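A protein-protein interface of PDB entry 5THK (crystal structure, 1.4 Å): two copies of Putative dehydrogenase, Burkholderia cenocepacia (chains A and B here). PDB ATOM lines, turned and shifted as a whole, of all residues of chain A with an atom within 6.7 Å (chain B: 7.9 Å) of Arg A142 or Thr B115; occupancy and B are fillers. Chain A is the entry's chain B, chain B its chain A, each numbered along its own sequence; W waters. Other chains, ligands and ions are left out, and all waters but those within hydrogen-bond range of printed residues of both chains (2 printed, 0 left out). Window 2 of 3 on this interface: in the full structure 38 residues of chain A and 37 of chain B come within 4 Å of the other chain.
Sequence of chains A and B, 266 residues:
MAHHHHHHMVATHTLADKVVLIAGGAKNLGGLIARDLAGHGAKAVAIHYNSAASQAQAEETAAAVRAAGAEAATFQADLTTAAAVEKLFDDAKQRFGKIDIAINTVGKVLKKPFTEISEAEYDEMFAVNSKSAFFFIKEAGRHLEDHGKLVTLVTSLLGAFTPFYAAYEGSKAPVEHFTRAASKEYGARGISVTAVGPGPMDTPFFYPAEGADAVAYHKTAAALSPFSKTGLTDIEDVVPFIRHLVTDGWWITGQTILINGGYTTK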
ATOM      1  N   LYS A  93     -10.087   6.533 -16.230  1.00  0.00           N
ATOM      2  CA  LYS A  93      -9.831   6.959 -17.602  1.00  0.00           C
ATOM      3  C   LYS A  93     -10.727   6.225 -18.598  1.00  0.00           C
ATOM      4  O   LYS A  93     -11.204   6.829 -19.569  1.00  0.00           O
ATOM      5  CB  LYS A  93      -8.349   6.773 -17.934  1.00  0.00           C
ATOM      6  CG  LYS A  93      -7.964   7.188 -19.346  1.00  0.00           C
ATOM      7  CD  LYS A  93      -6.444   7.258 -19.528  1.00  0.00           C
ATOM      8  CE  LYS A  93      -5.863   8.488 -18.840  1.00  0.00           C
ATOM      9  NZ  LYS A  93      -4.424   8.685 -19.180  1.00  0.00           N
ATOM     10  N   ILE A 137       0.653   9.210  -6.526  1.00  0.00           N
ATOM     11  CA  ILE A 137       1.461  10.256  -7.157  1.00  0.00           C
ATOM     12  C   ILE A 137       2.148   9.732  -8.414  1.00  0.00           C
ATOM     13  O   ILE A 137       2.201  10.427  -9.439  1.00  0.00           O
ATOM     14  CB  ILE A 137       2.459  10.858  -6.147  1.00  0.00           C
ATOM     15  CG1 ILE A 137       1.702  11.707  -5.120  1.00  0.00           C
ATOM     16  CG2 ILE A 137       3.519  11.701  -6.843  1.00  0.00           C
ATOM     17  CD1 ILE A 137       2.509  12.032  -3.883  1.00  0.00           C
ATOM     18  N   LYS A 138       2.676   8.501  -8.367  1.00  0.00           N
ATOM     19  CA  LYS A 138       3.308   7.917  -9.548  1.00  0.00           C
ATOM     20  C   LYS A 138       2.313   7.799 -10.697  1.00  0.00           C
ATOM     21  O   LYS A 138       2.595   8.211 -11.830  1.00  0.00           O
ATOM     22  CB  LYS A 138       3.869   6.537  -9.208  1.00  0.00           C
ATOM     23  CG  LYS A 138       4.430   5.794 -10.419  1.00  0.00           C
ATOM     24  CD  LYS A 138       4.805   4.350 -10.104  1.00  0.00           C
ATOM     25  CE  LYS A 138       5.228   3.620 -11.375  1.00  0.00           C
ATOM     26  NZ  LYS A 138       5.492   2.168 -11.128  1.00  0.00           N
ATOM     27  N   GLU A 139       1.144   7.214 -10.423  1.00  0.00           N
ATOM     28  CA  GLU A 139       0.172   6.987 -11.485  1.00  0.00           C
ATOM     29  C   GLU A 139      -0.425   8.294 -11.996  1.00  0.00           C
ATOM     30  O   GLU A 139      -0.735   8.407 -13.187  1.00  0.00           O
ATOM     31  CB  GLU A 139      -0.895   5.989 -11.025  1.00  0.00           C
ATOM     32  CG  GLU A 139      -0.355   4.580 -10.842  1.00  0.00           C
ATOM     33  CD  GLU A 139       0.330   4.060 -12.094  1.00  0.00           C
ATOM     34  OE1 GLU A 139      -0.240   4.212 -13.198  1.00  0.00           O
ATOM     35  OE2 GLU A 139       1.449   3.501 -11.980  1.00  0.00           O
ATOM     36  N   ALA A 140      -0.571   9.295 -11.129  1.00  0.00           N
ATOM     37  CA  ALA A 140      -0.984  10.613 -11.604  1.00  0.00           C
ATOM     38  C   ALA A 140       0.053  11.190 -12.557  1.00  0.00           C
ATOM     39  O   ALA A 140      -0.298  11.826 -13.561  1.00  0.00           O
ATOM     40  CB  ALA A 140      -1.216  11.562 -10.426  1.00  0.00           C
ATOM     41  N   GLY A 141       1.335  10.959 -12.272  1.00  0.00           N
ATOM     42  CA  GLY A 141       2.370  11.381 -13.199  1.00  0.00           C
ATOM     43  C   GLY A 141       2.256  10.717 -14.556  1.00  0.00           C
ATOM     44  O   GLY A 141       2.613  11.315 -15.575  1.00  0.00           O
ATOM     45  N   ARG A 142       1.757   9.478 -14.590  1.00  0.00           N
ATOM     46  CA  ARG A 142       1.615   8.764 -15.853  1.00  0.00           C
ATOM     47  C   ARG A 142       0.328   9.133 -16.582  1.00  0.00           C
ATOM     48  O   ARG A 142       0.264   9.016 -17.811  1.00  0.00           O
ATOM     49  CB  ARG A 142       1.670   7.254 -15.601  1.00  0.00           C
ATOM     50  CG  ARG A 142       2.987   6.783 -14.988  1.00  0.00           C
ATOM     51  CD  ARG A 142       3.057   5.268 -14.836  1.00  0.00           C
ATOM     52  NE  ARG A 142       3.067   4.600 -16.129  1.00  0.00           N
ATOM     53  CZ  ARG A 142       4.128   4.531 -16.930  1.00  0.00           C
ATOM     54  NH1 ARG A 142       5.277   5.091 -16.573  1.00  0.00           N
ATOM     55  NH2 ARG A 142       4.038   3.901 -18.094  1.00  0.00           N
ATOM     56  N   HIS A 143      -0.701   9.570 -15.856  1.00  0.00           N
ATOM     57  CA  HIS A 143      -2.036   9.691 -16.422  1.00  0.00           C
ATOM     58  C   HIS A 143      -2.571  11.104 -16.540  1.00  0.00           C
ATOM     59  O   HIS A 143      -3.450  11.335 -17.376  1.00  0.00           O
ATOM     60  CB  HIS A 143      -3.038   8.916 -15.568  1.00  0.00           C
ATOM     61  CG  HIS A 143      -3.063   7.454 -15.846  1.00  0.00           C
ATOM     62  ND1 HIS A 143      -3.763   6.917 -16.902  1.00  0.00           N
ATOM     63  CD2 HIS A 143      -2.496   6.413 -15.194  1.00  0.00           C
ATOM     64  CE1 HIS A 143      -3.617   5.605 -16.897  1.00  0.00           C
ATOM     65  NE2 HIS A 143      -2.856   5.274 -15.870  1.00  0.00           N
ATOM     66  N   LEU A 144      -2.132  12.036 -15.701  1.00  0.00           N
ATOM     67  CA  LEU A 144      -2.742  13.358 -15.703  1.00  0.00           C
ATOM     68  C   LEU A 144      -2.538  14.035 -17.048  1.00  0.00           C
ATOM     69  O   LEU A 144      -1.492  13.886 -17.686  1.00  0.00           O
ATOM     70  CB  LEU A 144      -2.112  14.233 -14.625  1.00  0.00           C
ATOM     71  CG  LEU A 144      -2.637  14.047 -13.207  1.00  0.00           C
ATOM     72  CD1 LEU A 144      -1.765  14.823 -12.249  1.00  0.00           C
ATOM     73  CD2 LEU A 144      -4.091  14.518 -13.113  1.00  0.00           C
ATOM     74  N   GLU A 185       9.554  17.012 -11.073  1.00  0.00           N
ATOM     75  CA  GLU A 185       9.547  16.140 -12.242  1.00  0.00           C
ATOM     76  C   GLU A 185       8.337  16.372 -13.133  1.00  0.00           C
ATOM     77  O   GLU A 185       8.437  16.215 -14.354  1.00  0.00           O
ATOM     78  CB  GLU A 185       9.620  14.674 -11.810  1.00  0.00           C
ATOM     79  CG  GLU A 185      10.919  14.324 -11.064  1.00  0.00           C
ATOM     80  CD  GLU A 185      11.011  12.862 -10.689  1.00  0.00           C
ATOM     81  OE1 GLU A 185      10.665  12.006 -11.531  1.00  0.00           O
ATOM     82  OE2 GLU A 185      11.437  12.572  -9.548  1.00  0.00           O
ATOM     83  N   TYR A 186       7.196  16.739 -12.551  1.00  0.00           N
ATOM     84  CA  TYR A 186       5.969  16.892 -13.328  1.00  0.00           C
ATOM     85  C   TYR A 186       5.748  18.325 -13.804  1.00  0.00           C
ATOM     86  O   TYR A 186       4.851  18.557 -14.627  1.00  0.00           O
ATOM     87  CB  TYR A 186       4.730  16.441 -12.526  1.00  0.00           C
ATOM     88  CG  TYR A 186       4.724  15.000 -12.012  1.00  0.00           C
ATOM     89  CD1 TYR A 186       5.686  14.065 -12.400  1.00  0.00           C
ATOM     90  CD2 TYR A 186       3.737  14.582 -11.124  1.00  0.00           C
ATOM     91  CE1 TYR A 186       5.660  12.759 -11.903  1.00  0.00           C
ATOM     92  CE2 TYR A 186       3.708  13.287 -10.620  1.00  0.00           C
ATOM     93  CZ  TYR A 186       4.669  12.379 -11.016  1.00  0.00           C
ATOM     94  OH  TYR A 186       4.645  11.087 -10.535  1.00  0.00           O
ATOM     95  N   ARG A 189       5.332  19.344 -17.548  1.00  0.00           N
ATOM     96  CA  ARG A 189       4.031  19.193 -18.188  1.00  0.00           C
ATOM     97  C   ARG A 189       2.993  20.158 -17.632  1.00  0.00           C
ATOM     98  O   ARG A 189       1.802  20.019 -17.935  1.00  0.00           O
ATOM     99  CB  ARG A 189       3.516  17.758 -18.036  1.00  0.00           C
ATOM    100  CG  ARG A 189       4.446  16.703 -18.581  1.00  0.00           C
ATOM    101  CD  ARG A 189       3.677  15.501 -19.089  1.00  0.00           C
ATOM    102  NE  ARG A 189       3.082  14.649 -18.054  1.00  0.00           N
ATOM    103  CZ  ARG A 189       1.771  14.455 -17.908  1.00  0.00           C
ATOM    104  NH1 ARG A 189       0.907  15.078 -18.702  1.00  0.00           N
ATOM    105  NH2 ARG A 189       1.320  13.627 -16.969  1.00  0.00           N
ATOM    106  N   LYS B 112      15.926   7.699  -9.327  1.00  0.00           N
ATOM    107  CA  LYS B 112      15.180   7.272 -10.505  1.00  0.00           C
ATOM    108  C   LYS B 112      13.964   8.170 -10.693  1.00  0.00           C
ATOM    109  O   LYS B 112      13.390   8.638  -9.698  1.00  0.00           O
ATOM    110  CB  LYS B 112      14.727   5.824 -10.277  1.00  0.00           C
ATOM    111  CG  LYS B 112      13.907   5.203 -11.386  1.00  0.00           C
ATOM    112  CD  LYS B 112      13.669   3.720 -11.135  1.00  0.00           C
ATOM    113  CE  LYS B 112      14.732   2.864 -11.788  1.00  0.00           C
ATOM    114  NZ  LYS B 112      14.297   1.443 -11.878  1.00  0.00           N
ATOM    115  N   PRO B 113      13.537   8.435 -11.932  1.00  0.00           N
ATOM    116  CA  PRO B 113      12.291   9.189 -12.134  1.00  0.00           C
ATOM    117  C   PRO B 113      11.113   8.511 -11.447  1.00  0.00           C
ATOM    118  O   PRO B 113      10.974   7.286 -11.477  1.00  0.00           O
ATOM    119  CB  PRO B 113      12.122   9.177 -13.658  1.00  0.00           C
ATOM    120  CG  PRO B 113      13.519   9.043 -14.181  1.00  0.00           C
ATOM    121  CD  PRO B 113      14.210   8.131 -13.211  1.00  0.00           C
ATOM    122  N   PHE B 114      10.256   9.338 -10.837  1.00  0.00           N
ATOM    123  CA  PHE B 114       9.097   8.854 -10.087  1.00  0.00           C
ATOM    124  C   PHE B 114       8.270   7.858 -10.905  1.00  0.00           C
ATOM    125  O   PHE B 114       7.893   6.789 -10.406  1.00  0.00           O
ATOM    126  CB  PHE B 114       8.253  10.075  -9.672  1.00  0.00           C
ATOM    127  CG  PHE B 114       7.558   9.949  -8.319  1.00  0.00           C
ATOM    128  CD1 PHE B 114       6.825   8.814  -7.981  1.00  0.00           C
ATOM    129  CD2 PHE B 114       7.609  10.998  -7.403  1.00  0.00           C
ATOM    130  CE1 PHE B 114       6.167   8.710  -6.747  1.00  0.00           C
ATOM    131  CE2 PHE B 114       6.965  10.894  -6.167  1.00  0.00           C
ATOM    132  CZ  PHE B 114       6.241   9.752  -5.840  1.00  0.00           C
ATOM    133  N   THR B 115       8.010   8.164 -12.180  1.00  0.00           N
ATOM    134  CA  THR B 115       7.123   7.309 -12.968  1.00  0.00           C
ATOM    135  C   THR B 115       7.739   5.964 -13.321  1.00  0.00           C
ATOM    136  O   THR B 115       7.028   5.107 -13.861  1.00  0.00           O
ATOM    137  CB  THR B 115       6.676   8.018 -14.247  1.00  0.00           C
ATOM    138  OG1 THR B 115       7.829   8.475 -14.965  1.00  0.00           O
ATOM    139  CG2 THR B 115       5.759   9.194 -13.920  1.00  0.00           C
ATOM    140  N   GLU B 116       9.021   5.750 -13.028  1.00  0.00           N
ATOM    141  CA  GLU B 116       9.685   4.486 -13.314  1.00  0.00           C
ATOM    142  C   GLU B 116       9.885   3.600 -12.093  1.00  0.00           C
ATOM    143  O   GLU B 116      10.356   2.467 -12.245  1.00  0.00           O
ATOM    144  CB  GLU B 116      11.058   4.735 -13.937  1.00  0.00           C
ATOM    145  CG  GLU B 116      11.028   5.339 -15.312  1.00  0.00           C
ATOM    146  CD  GLU B 116      12.417   5.377 -15.902  1.00  0.00           C
ATOM    147  OE1 GLU B 116      12.906   6.479 -16.211  1.00  0.00           O
ATOM    148  OE2 GLU B 116      13.031   4.293 -16.040  1.00  0.00           O
ATOM    149  N   ILE B 117       9.565   4.074 -10.895  1.00  0.00           N
ATOM    150  CA  ILE B 117       9.876   3.316  -9.688  1.00  0.00           C
ATOM    151  C   ILE B 117       8.854   2.199  -9.505  1.00  0.00           C
ATOM    152  O   ILE B 117       7.648   2.448  -9.415  1.00  0.00           O
ATOM    153  CB  ILE B 117       9.947   4.230  -8.460  1.00  0.00           C
ATOM    154  CG1 ILE B 117      11.102   5.228  -8.621  1.00  0.00           C
ATOM    155  CG2 ILE B 117      10.133   3.400  -7.199  1.00  0.00           C
ATOM    156  CD1 ILE B 117      11.120   6.328  -7.559  1.00  0.00           C
ATOM    157  N   SER B 118       9.339   0.967  -9.435  1.00  0.00           N
ATOM    158  CA  SER B 118       8.478  -0.199  -9.370  1.00  0.00           C
ATOM    159  C   SER B 118       8.016  -0.452  -7.935  1.00  0.00           C
ATOM    160  O   SER B 118       8.561   0.082  -6.965  1.00  0.00           O
ATOM    161  CB  SER B 118       9.226  -1.430  -9.871  1.00  0.00           C
ATOM    162  OG  SER B 118      10.269  -1.758  -8.965  1.00  0.00           O
ATOM    163  N   ALA B 166      12.670  10.477  -4.835  1.00  0.00           N
ATOM    164  CA  ALA B 166      11.404  10.348  -4.111  1.00  0.00           C
ATOM    165  C   ALA B 166      11.407   9.167  -3.151  1.00  0.00           C
ATOM    166  O   ALA B 166      10.925   9.282  -2.019  1.00  0.00           O
ATOM    167  CB  ALA B 166      10.232  10.246  -5.088  1.00  0.00           C
HETATM  168  O   HOH W   1       8.536  10.987 -13.060  1.00  0.00           O
HETATM  169  O   HOH W   2      11.945  10.382  -7.837  1.00  0.00           O
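Glu A139 touches none of the printed residues of chain B. Of chain B, only Thr B115 (3.2 Å) comes within 4 Å of Arg A142. Of the printed residues of chain B, Glu A185 touches Pro B113 and Phe B114. Of the printed residues of chain B, Tyr A186 touches Phe B114 (3.8 Å). Printed residues of chain A within 4 Å of Pro B113: Glu A185 (3.3 Å). Printed residues of chain A within 4 Å of Phe B114: Ile A137 (3.5 Å), Lys A138 (3.6 Å), Glu A185 (2.8 Å) and Tyr A186 (3.8 Å). Of the printed residues of chain A, Thr B115 touches Lys A138 (3.4 Å), Gly A141 (3.9 Å) and Arg A142 (3.2 Å). The nearest residue of chain B that does not touch Arg A142 is Glu B116 (5.2 Å). The nearest printed residue of chain B that does not touch Lys A138 is Ser B118 (4.2 Å).
Phe B114 touches Ile A137. Lys A138 touches Phe B114 (CG to O, 3.6 Å). Thr B115 touches Lys A138 (O to CE, 3.4 Å). C of Gly A141 touches CG2 of Thr B115, at 3.9 Å. OE1 of Glu A185 touches CA of Pro B113, at 3.3 Å. Phe B114 touches Tyr A186 (CG to OH, 3.8 Å).
The backbone NH (N) of Phe B114 sits at hydrogen-bond distance from the side-chain carboxylate (OE1) of Glu A185, at 2.8 Å. O of Thr B115 is in hydrogen-bond range of NH1 of Arg A142 (3.2 Å). The backbone carbonyl oxygen (O) of Ile B117 sits at hydrogen-bond distance from the side-chain amino group (NZ) of Lys A138 (2.8 Å).
The side-chain hydroxyl (OH) of Tyr A186 lies within hydrogen-bond range of the backbone carbonyl oxygen (O) of Ile A137, 2.8 Å away. The guanidinium group (NH2) of Arg A189 is in hydrogen-bond range of the backbone carbonyl oxygen (O) of Gly A141.
Among the printed residues, 9 pairs touch across the chains. Among the printed residues, no Asp or Glu carboxylate lies within 4 Å of a Lys or Arg side-chain nitrogen of the other chain.
Water W1 lies within hydrogen-bond range of OE1 of Glu A185 (2.8 Å), N of Thr B115 (3.0 Å) and N of Phe B114 (3.3 Å). Water W2 lies within hydrogen-bond range of the side-chain carboxylate (OE2) of Glu A185 (2.8 Å), the backbone carbonyl oxygen (O) of Lys B112 (2.9 Å) and the backbone NH (N) of Ala B166 (3.1 Å).
No position is printed for both chains. Of the 9 pairs that touch across the chains among the printed residues, none has its exchanged pair printed and touching as well.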
